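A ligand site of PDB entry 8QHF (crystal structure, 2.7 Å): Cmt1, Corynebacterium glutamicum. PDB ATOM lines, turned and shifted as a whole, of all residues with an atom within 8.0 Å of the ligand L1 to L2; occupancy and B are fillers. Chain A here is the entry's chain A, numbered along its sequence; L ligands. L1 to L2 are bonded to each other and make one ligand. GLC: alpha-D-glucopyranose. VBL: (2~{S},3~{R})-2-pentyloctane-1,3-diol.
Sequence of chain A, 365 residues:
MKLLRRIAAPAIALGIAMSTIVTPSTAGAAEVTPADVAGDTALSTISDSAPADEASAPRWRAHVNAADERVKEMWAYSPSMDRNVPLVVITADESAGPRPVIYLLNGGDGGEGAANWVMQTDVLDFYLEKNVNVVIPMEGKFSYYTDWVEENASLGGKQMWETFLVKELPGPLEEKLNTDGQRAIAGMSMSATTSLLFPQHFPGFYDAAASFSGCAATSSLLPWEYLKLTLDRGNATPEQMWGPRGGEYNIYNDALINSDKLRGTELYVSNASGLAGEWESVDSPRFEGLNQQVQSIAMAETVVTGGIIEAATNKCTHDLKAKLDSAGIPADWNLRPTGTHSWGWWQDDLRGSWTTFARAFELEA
An oxygen (O4) of GLC L1 sits at hydrogen-bond distance from the side-chain carboxylate (OE1) of Glu 225 (2.9 Å). OD2 of Asp 232 is in hydrogen-bond range of O2 of GLC L1, at 3.0 Å.
Merely in contact with the ligand L1 to L2: Leu 229 and Lys 228. Hydrophobic or aromatic side chains that line the ligand L1 to L2: Leu 229.
The side-chain carboxylate (OE1) of Glu 225 is in salt-bridge range of the side-chain amino group (NZ) of Lys 228, at 2.7 Å.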
ATOM      1  N   LEU A 221      -8.752 -40.503  25.387  1.00  0.00           N
ATOM      2  CA  LEU A 221      -7.705 -39.569  24.980  1.00  0.00           C
ATOM      3  C   LEU A 221      -8.108 -38.103  25.071  1.00  0.00           C
ATOM      4  O   LEU A 221      -7.486 -37.356  25.818  1.00  0.00           O
ATOM      5  CB  LEU A 221      -7.241 -39.940  23.575  1.00  0.00           C
ATOM      6  CG  LEU A 221      -5.900 -39.368  23.174  1.00  0.00           C
ATOM      7  CD1 LEU A 221      -4.782 -40.318  23.565  1.00  0.00           C
ATOM      8  CD2 LEU A 221      -5.877 -39.040  21.680  1.00  0.00           C
ATOM      9  N   LEU A 222      -9.147 -37.692  24.346  1.00  0.00           N
ATOM     10  CA  LEU A 222      -9.611 -36.323  24.379  1.00  0.00           C
ATOM     11  C   LEU A 222     -10.203 -35.966  25.735  1.00  0.00           C
ATOM     12  O   LEU A 222      -9.716 -35.002  26.311  1.00  0.00           O
ATOM     13  CB  LEU A 222     -10.565 -36.020  23.228  1.00  0.00           C
ATOM     14  CG  LEU A 222      -9.919 -35.738  21.876  1.00  0.00           C
ATOM     15  CD1 LEU A 222     -10.975 -35.483  20.837  1.00  0.00           C
ATOM     16  CD2 LEU A 222      -8.959 -34.556  21.954  1.00  0.00           C
ATOM     17  N   PRO A 223     -11.151 -36.746  26.318  1.00  0.00           N
ATOM     18  CA  PRO A 223     -11.683 -36.391  27.646  1.00  0.00           C
ATOM     19  C   PRO A 223     -10.657 -36.216  28.767  1.00  0.00           C
ATOM     20  O   PRO A 223     -10.885 -35.398  29.652  1.00  0.00           O
ATOM     21  CB  PRO A 223     -12.646 -37.537  27.932  1.00  0.00           C
ATOM     22  CG  PRO A 223     -13.124 -37.952  26.595  1.00  0.00           C
ATOM     23  CD  PRO A 223     -11.886 -37.891  25.756  1.00  0.00           C
ATOM     24  N   TRP A 224      -9.542 -36.951  28.721  1.00  0.00           N
ATOM     25  CA  TRP A 224      -8.483 -36.785  29.717  1.00  0.00           C
ATOM     26  C   TRP A 224      -7.816 -35.409  29.551  1.00  0.00           C
ATOM     27  O   TRP A 224      -7.460 -34.755  30.537  1.00  0.00           O
ATOM     28  CB  TRP A 224      -7.425 -37.886  29.557  1.00  0.00           C
ATOM     29  CG  TRP A 224      -6.268 -37.794  30.504  1.00  0.00           C
ATOM     30  CD1 TRP A 224      -5.040 -37.270  30.245  1.00  0.00           C
ATOM     31  CD2 TRP A 224      -6.205 -38.324  31.841  1.00  0.00           C
ATOM     32  NE1 TRP A 224      -4.220 -37.396  31.351  1.00  0.00           N
ATOM     33  CE2 TRP A 224      -4.918 -38.032  32.340  1.00  0.00           C
ATOM     34  CE3 TRP A 224      -7.121 -38.959  32.686  1.00  0.00           C
ATOM     35  CZ2 TRP A 224      -4.514 -38.414  33.623  1.00  0.00           C
ATOM     36  CZ3 TRP A 224      -6.724 -39.321  33.963  1.00  0.00           C
ATOM     37  CH2 TRP A 224      -5.442 -39.028  34.420  1.00  0.00           C
ATOM     38  N   GLU A 225      -7.656 -34.959  28.312  1.00  0.00           N
ATOM     39  CA  GLU A 225      -7.081 -33.667  28.013  1.00  0.00           C
ATOM     40  C   GLU A 225      -8.001 -32.525  28.456  1.00  0.00           C
ATOM     41  O   GLU A 225      -7.500 -31.459  28.825  1.00  0.00           O
ATOM     42  CB  GLU A 225      -6.746 -33.601  26.525  1.00  0.00           C
ATOM     43  CG  GLU A 225      -5.780 -34.695  26.092  1.00  0.00           C
ATOM     44  CD  GLU A 225      -4.407 -34.638  26.726  1.00  0.00           C
ATOM     45  OE1 GLU A 225      -3.951 -33.520  27.059  1.00  0.00           O
ATOM     46  OE2 GLU A 225      -3.771 -35.706  26.884  1.00  0.00           O
ATOM     47  N   TYR A 226      -9.321 -32.742  28.461  1.00  0.00           N
ATOM     48  CA  TYR A 226     -10.276 -31.740  28.955  1.00  0.00           C
ATOM     49  C   TYR A 226     -10.149 -31.554  30.468  1.00  0.00           C
ATOM     50  O   TYR A 226     -10.463 -30.487  30.990  1.00  0.00           O
ATOM     51  CB  TYR A 226     -11.714 -32.139  28.645  1.00  0.00           C
ATOM     52  CG  TYR A 226     -12.030 -32.549  27.230  1.00  0.00           C
ATOM     53  CD1 TYR A 226     -11.298 -32.054  26.156  1.00  0.00           C
ATOM     54  CD2 TYR A 226     -13.151 -33.311  26.944  1.00  0.00           C
ATOM     55  CE1 TYR A 226     -11.614 -32.405  24.842  1.00  0.00           C
ATOM     56  CE2 TYR A 226     -13.465 -33.683  25.644  1.00  0.00           C
ATOM     57  CZ  TYR A 226     -12.703 -33.219  24.594  1.00  0.00           C
ATOM     58  OH  TYR A 226     -13.071 -33.569  23.316  1.00  0.00           O
ATOM     59  N   LEU A 227      -9.718 -32.601  31.201  1.00  0.00           N
ATOM     60  CA  LEU A 227      -9.475 -32.489  32.641  1.00  0.00           C
ATOM     61  C   LEU A 227      -8.351 -31.466  32.874  1.00  0.00           C
ATOM     62  O   LEU A 227      -8.448 -30.642  33.770  1.00  0.00           O
ATOM     63  CB  LEU A 227      -9.088 -33.873  33.245  1.00  0.00           C
ATOM     64  CG  LEU A 227     -10.109 -35.012  33.132  1.00  0.00           C
ATOM     65  CD1 LEU A 227      -9.640 -36.241  33.885  1.00  0.00           C
ATOM     66  CD2 LEU A 227     -11.475 -34.624  33.660  1.00  0.00           C
ATOM     67  N   LYS A 228      -7.320 -31.466  32.003  1.00  0.00           N
ATOM     68  CA  LYS A 228      -6.211 -30.529  32.022  1.00  0.00           C
ATOM     69  C   LYS A 228      -6.662 -29.058  31.848  1.00  0.00           C
ATOM     70  O   LYS A 228      -6.078 -28.209  32.488  1.00  0.00           O
ATOM     71  CB  LYS A 228      -5.135 -30.910  31.003  1.00  0.00           C
ATOM     72  CG  LYS A 228      -4.499 -32.250  31.306  1.00  0.00           C
ATOM     73  CD  LYS A 228      -3.496 -32.617  30.268  1.00  0.00           C
ATOM     74  CE  LYS A 228      -3.035 -34.029  30.449  1.00  0.00           C
ATOM     75  NZ  LYS A 228      -2.608 -34.641  29.159  1.00  0.00           N
ATOM     76  N   LEU A 229      -7.706 -28.746  31.059  1.00  0.00           N
ATOM     77  CA  LEU A 229      -8.182 -27.354  30.929  1.00  0.00           C
ATOM     78  C   LEU A 229      -8.576 -26.776  32.322  1.00  0.00           C
ATOM     79  O   LEU A 229      -8.225 -25.653  32.675  1.00  0.00           O
ATOM     80  CB  LEU A 229      -9.416 -27.253  29.996  1.00  0.00           C
ATOM     81  CG  LEU A 229      -9.223 -26.862  28.531  1.00  0.00           C
ATOM     82  CD1 LEU A 229      -8.346 -25.634  28.379  1.00  0.00           C
ATOM     83  CD2 LEU A 229      -8.726 -28.033  27.735  1.00  0.00           C
ATOM     84  N   THR A 230      -9.300 -27.587  33.104  1.00  0.00           N
ATOM     85  CA  THR A 230      -9.753 -27.176  34.416  1.00  0.00           C
ATOM     86  C   THR A 230      -8.633 -27.223  35.450  1.00  0.00           C
ATOM     87  O   THR A 230      -8.421 -26.250  36.154  1.00  0.00           O
ATOM     88  CB  THR A 230     -10.954 -28.044  34.830  1.00  0.00           C
ATOM     89  OG1 THR A 230     -11.991 -27.900  33.858  1.00  0.00           O
ATOM     90  CG2 THR A 230     -11.487 -27.669  36.193  1.00  0.00           C
ATOM     91  N   ASP A 232      -5.274 -27.273  35.120  1.00  0.00           N
ATOM     92  CA  ASP A 232      -4.128 -26.395  34.891  1.00  0.00           C
ATOM     93  C   ASP A 232      -4.307 -25.056  35.614  1.00  0.00           C
ATOM     94  O   ASP A 232      -3.322 -24.511  36.127  1.00  0.00           O
ATOM     95  CB  ASP A 232      -3.873 -26.176  33.402  1.00  0.00           C
ATOM     96  CG  ASP A 232      -3.150 -27.307  32.692  1.00  0.00           C
ATOM     97  OD1 ASP A 232      -2.870 -28.338  33.358  1.00  0.00           O
ATOM     98  OD2 ASP A 232      -2.885 -27.172  31.478  1.00  0.00           O
ATOM     99  N   ARG A 233      -5.553 -24.567  35.701  1.00  0.00           N
ATOM    100  CA  ARG A 233      -5.895 -23.321  36.401  1.00  0.00           C
ATOM    101  C   ARG A 233      -5.648 -23.390  37.922  1.00  0.00           C
ATOM    102  O   ARG A 233      -5.513 -22.363  38.565  1.00  0.00           O
ATOM    103  CB  ARG A 233      -7.335 -22.910  36.112  1.00  0.00           C
ATOM    104  CG  ARG A 233      -7.629 -22.589  34.650  1.00  0.00           C
ATOM    105  CD  ARG A 233      -7.500 -21.099  34.318  1.00  0.00           C
ATOM    106  NE  ARG A 233      -8.155 -20.214  35.300  1.00  0.00           N
ATOM    107  CZ  ARG A 233      -8.948 -19.198  34.983  1.00  0.00           C
ATOM    108  NH1 ARG A 233      -9.241 -18.940  33.713  1.00  0.00           N
ATOM    109  NH2 ARG A 233      -9.498 -18.457  35.935  1.00  0.00           N
ATOM    110  N   PRO A 238      -4.193 -34.095  36.146  1.00  0.00           N
ATOM    111  CA  PRO A 238      -5.208 -35.139  36.391  1.00  0.00           C
ATOM    112  C   PRO A 238      -4.643 -36.401  37.067  1.00  0.00           C
ATOM    113  O   PRO A 238      -5.406 -37.099  37.728  1.00  0.00           O
ATOM    114  CB  PRO A 238      -5.812 -35.387  35.015  1.00  0.00           C
ATOM    115  CG  PRO A 238      -4.789 -34.916  34.054  1.00  0.00           C
ATOM    116  CD  PRO A 238      -4.009 -33.834  34.702  1.00  0.00           C
ATOM    117  N   GLU A 301     -11.228 -14.503  19.928  1.00  0.00           N
ATOM    118  CA  GLU A 301     -10.771 -15.583  20.771  1.00  0.00           C
ATOM    119  C   GLU A 301     -11.913 -16.236  21.466  1.00  0.00           C
ATOM    120  O   GLU A 301     -11.882 -17.450  21.576  1.00  0.00           O
ATOM    121  CB  GLU A 301      -9.818 -15.054  21.829  1.00  0.00           C
ATOM    122  CG  GLU A 301      -8.569 -14.436  21.255  1.00  0.00           C
ATOM    123  CD  GLU A 301      -7.300 -15.004  21.870  1.00  0.00           C
ATOM    124  OE1 GLU A 301      -7.354 -15.427  23.038  1.00  0.00           O
ATOM    125  OE2 GLU A 301      -6.265 -15.027  21.155  1.00  0.00           O
ATOM    126  N   THR A 305     -12.539 -20.223  21.282  1.00  0.00           N
ATOM    127  CA  THR A 305     -12.493 -21.041  22.509  1.00  0.00           C
ATOM    128  C   THR A 305     -13.860 -21.602  22.928  1.00  0.00           C
ATOM    129  O   THR A 305     -13.953 -22.754  23.332  1.00  0.00           O
ATOM    130  CB  THR A 305     -11.896 -20.248  23.667  1.00  0.00           C
ATOM    131  OG1 THR A 305     -12.839 -19.275  24.095  1.00  0.00           O
ATOM    132  CG2 THR A 305     -10.575 -19.616  23.312  1.00  0.00           C
ATOM    133  N   ILE A 308     -14.577 -24.345  20.510  1.00  0.00           N
ATOM    134  CA  ILE A 308     -13.864 -25.589  20.833  1.00  0.00           C
ATOM    135  C   ILE A 308     -14.511 -26.249  22.065  1.00  0.00           C
ATOM    136  O   ILE A 308     -14.644 -27.466  22.110  1.00  0.00           O
ATOM    137  CB  ILE A 308     -12.342 -25.332  21.060  1.00  0.00           C
ATOM    138  CG1 ILE A 308     -11.637 -24.864  19.775  1.00  0.00           C
ATOM    139  CG2 ILE A 308     -11.654 -26.548  21.679  1.00  0.00           C
ATOM    140  CD1 ILE A 308     -10.292 -24.360  20.000  1.00  0.00           C
ATOM    141  N   ALA A 312     -16.416 -29.966  21.997  1.00  0.00           N
ATOM    142  CA  ALA A 312     -15.946 -30.997  22.925  1.00  0.00           C
ATOM    143  C   ALA A 312     -17.094 -31.563  23.779  1.00  0.00           C
ATOM    144  O   ALA A 312     -17.212 -32.780  23.886  1.00  0.00           O
ATOM    145  CB  ALA A 312     -14.856 -30.421  23.810  1.00  0.00           C
HETATM  146  C1  GLC L   1      -5.211 -27.735  27.077  1.00  0.00           C
HETATM  147  C2  GLC L   1      -4.143 -28.438  27.893  1.00  0.00           C
HETATM  148  C3  GLC L   1      -3.400 -29.437  27.019  1.00  0.00           C
HETATM  149  C4  GLC L   1      -4.363 -30.381  26.290  1.00  0.00           C
HETATM  150  C5  GLC L   1      -5.438 -29.597  25.505  1.00  0.00           C
HETATM  151  C6  GLC L   1      -6.517 -30.488  24.912  1.00  0.00           C
HETATM  152  O2  GLC L   1      -3.298 -27.489  28.530  1.00  0.00           O
HETATM  153  O3  GLC L   1      -2.498 -30.184  27.833  1.00  0.00           O
HETATM  154  O4  GLC L   1      -3.640 -31.189  25.372  1.00  0.00           O
HETATM  155  O5  GLC L   1      -6.093 -28.682  26.423  1.00  0.00           O
HETATM  156  O6  GLC L   1      -7.575 -29.757  24.281  1.00  0.00           O
HETATM  157  C1  GLC L   2      -5.090 -25.975  25.240  1.00  0.00           C
HETATM  158  C2  GLC L   2      -4.219 -25.664  24.024  1.00  0.00           C
HETATM  159  C3  GLC L   2      -3.121 -24.671  24.402  1.00  0.00           C
HETATM  160  C4  GLC L   2      -3.707 -23.436  25.089  1.00  0.00           C
HETATM  161  C5  GLC L   2      -4.581 -23.826  26.304  1.00  0.00           C
HETATM  162  C6  GLC L   2      -5.318 -22.674  26.952  1.00  0.00           C
HETATM  163  O1  GLC L   2      -4.458 -26.812  26.151  1.00  0.00           O
HETATM  164  O2  GLC L   2      -3.695 -26.858  23.452  1.00  0.00           O
HETATM  165  O3  GLC L   2      -2.401 -24.315  23.220  1.00  0.00           O
HETATM  166  O4  GLC L   2      -2.627 -22.624  25.545  1.00  0.00           O
HETATM  167  O5  GLC L   2      -5.593 -24.771  25.866  1.00  0.00           O
HETATM  168  O6  GLC L   2      -6.331 -22.113  26.106  1.00  0.00           O
HETATM  169  C3  VBL L   3     -15.863 -26.455  30.778  1.00  0.00           C
HETATM  170  C4  VBL L   3     -14.897 -25.247  31.113  1.00  0.00           C
HETATM  171  C5  VBL L   3     -13.806 -25.077  30.045  1.00  0.00           C
HETATM  172  C6  VBL L   3     -12.399 -24.770  30.586  1.00  0.00           C
HETATM  173  C7  VBL L   3     -12.228 -23.332  31.110  1.00  0.00           C
HETATM  174  C8  VBL L   3     -11.261 -23.245  32.301  1.00  0.00           C
HETATM  175  C9  VBL L   3     -11.907 -23.637  33.630  1.00  0.00           C
HETATM  176  C1  VBL L   3     -16.222 -28.925  30.152  1.00  0.00           C
HETATM  177  C2  VBL L   3     -15.259 -27.901  30.805  1.00  0.00           C
HETATM  178  C10 VBL L   3     -17.202 -26.432  31.574  1.00  0.00           C
HETATM  179  C12 VBL L   3     -14.647 -29.534  27.399  1.00  0.00           C
HETATM  180  C11 VBL L   3     -15.737 -30.340  28.099  1.00  0.00           C
HETATM  181  C   VBL L   3     -15.568 -30.206  29.620  1.00  0.00           C
HETATM  182  O   VBL L   3     -15.667 -24.054  31.038  1.00  0.00           O
HETATM  183  O1  VBL L   3     -18.211 -26.529  30.566  1.00  0.00           O
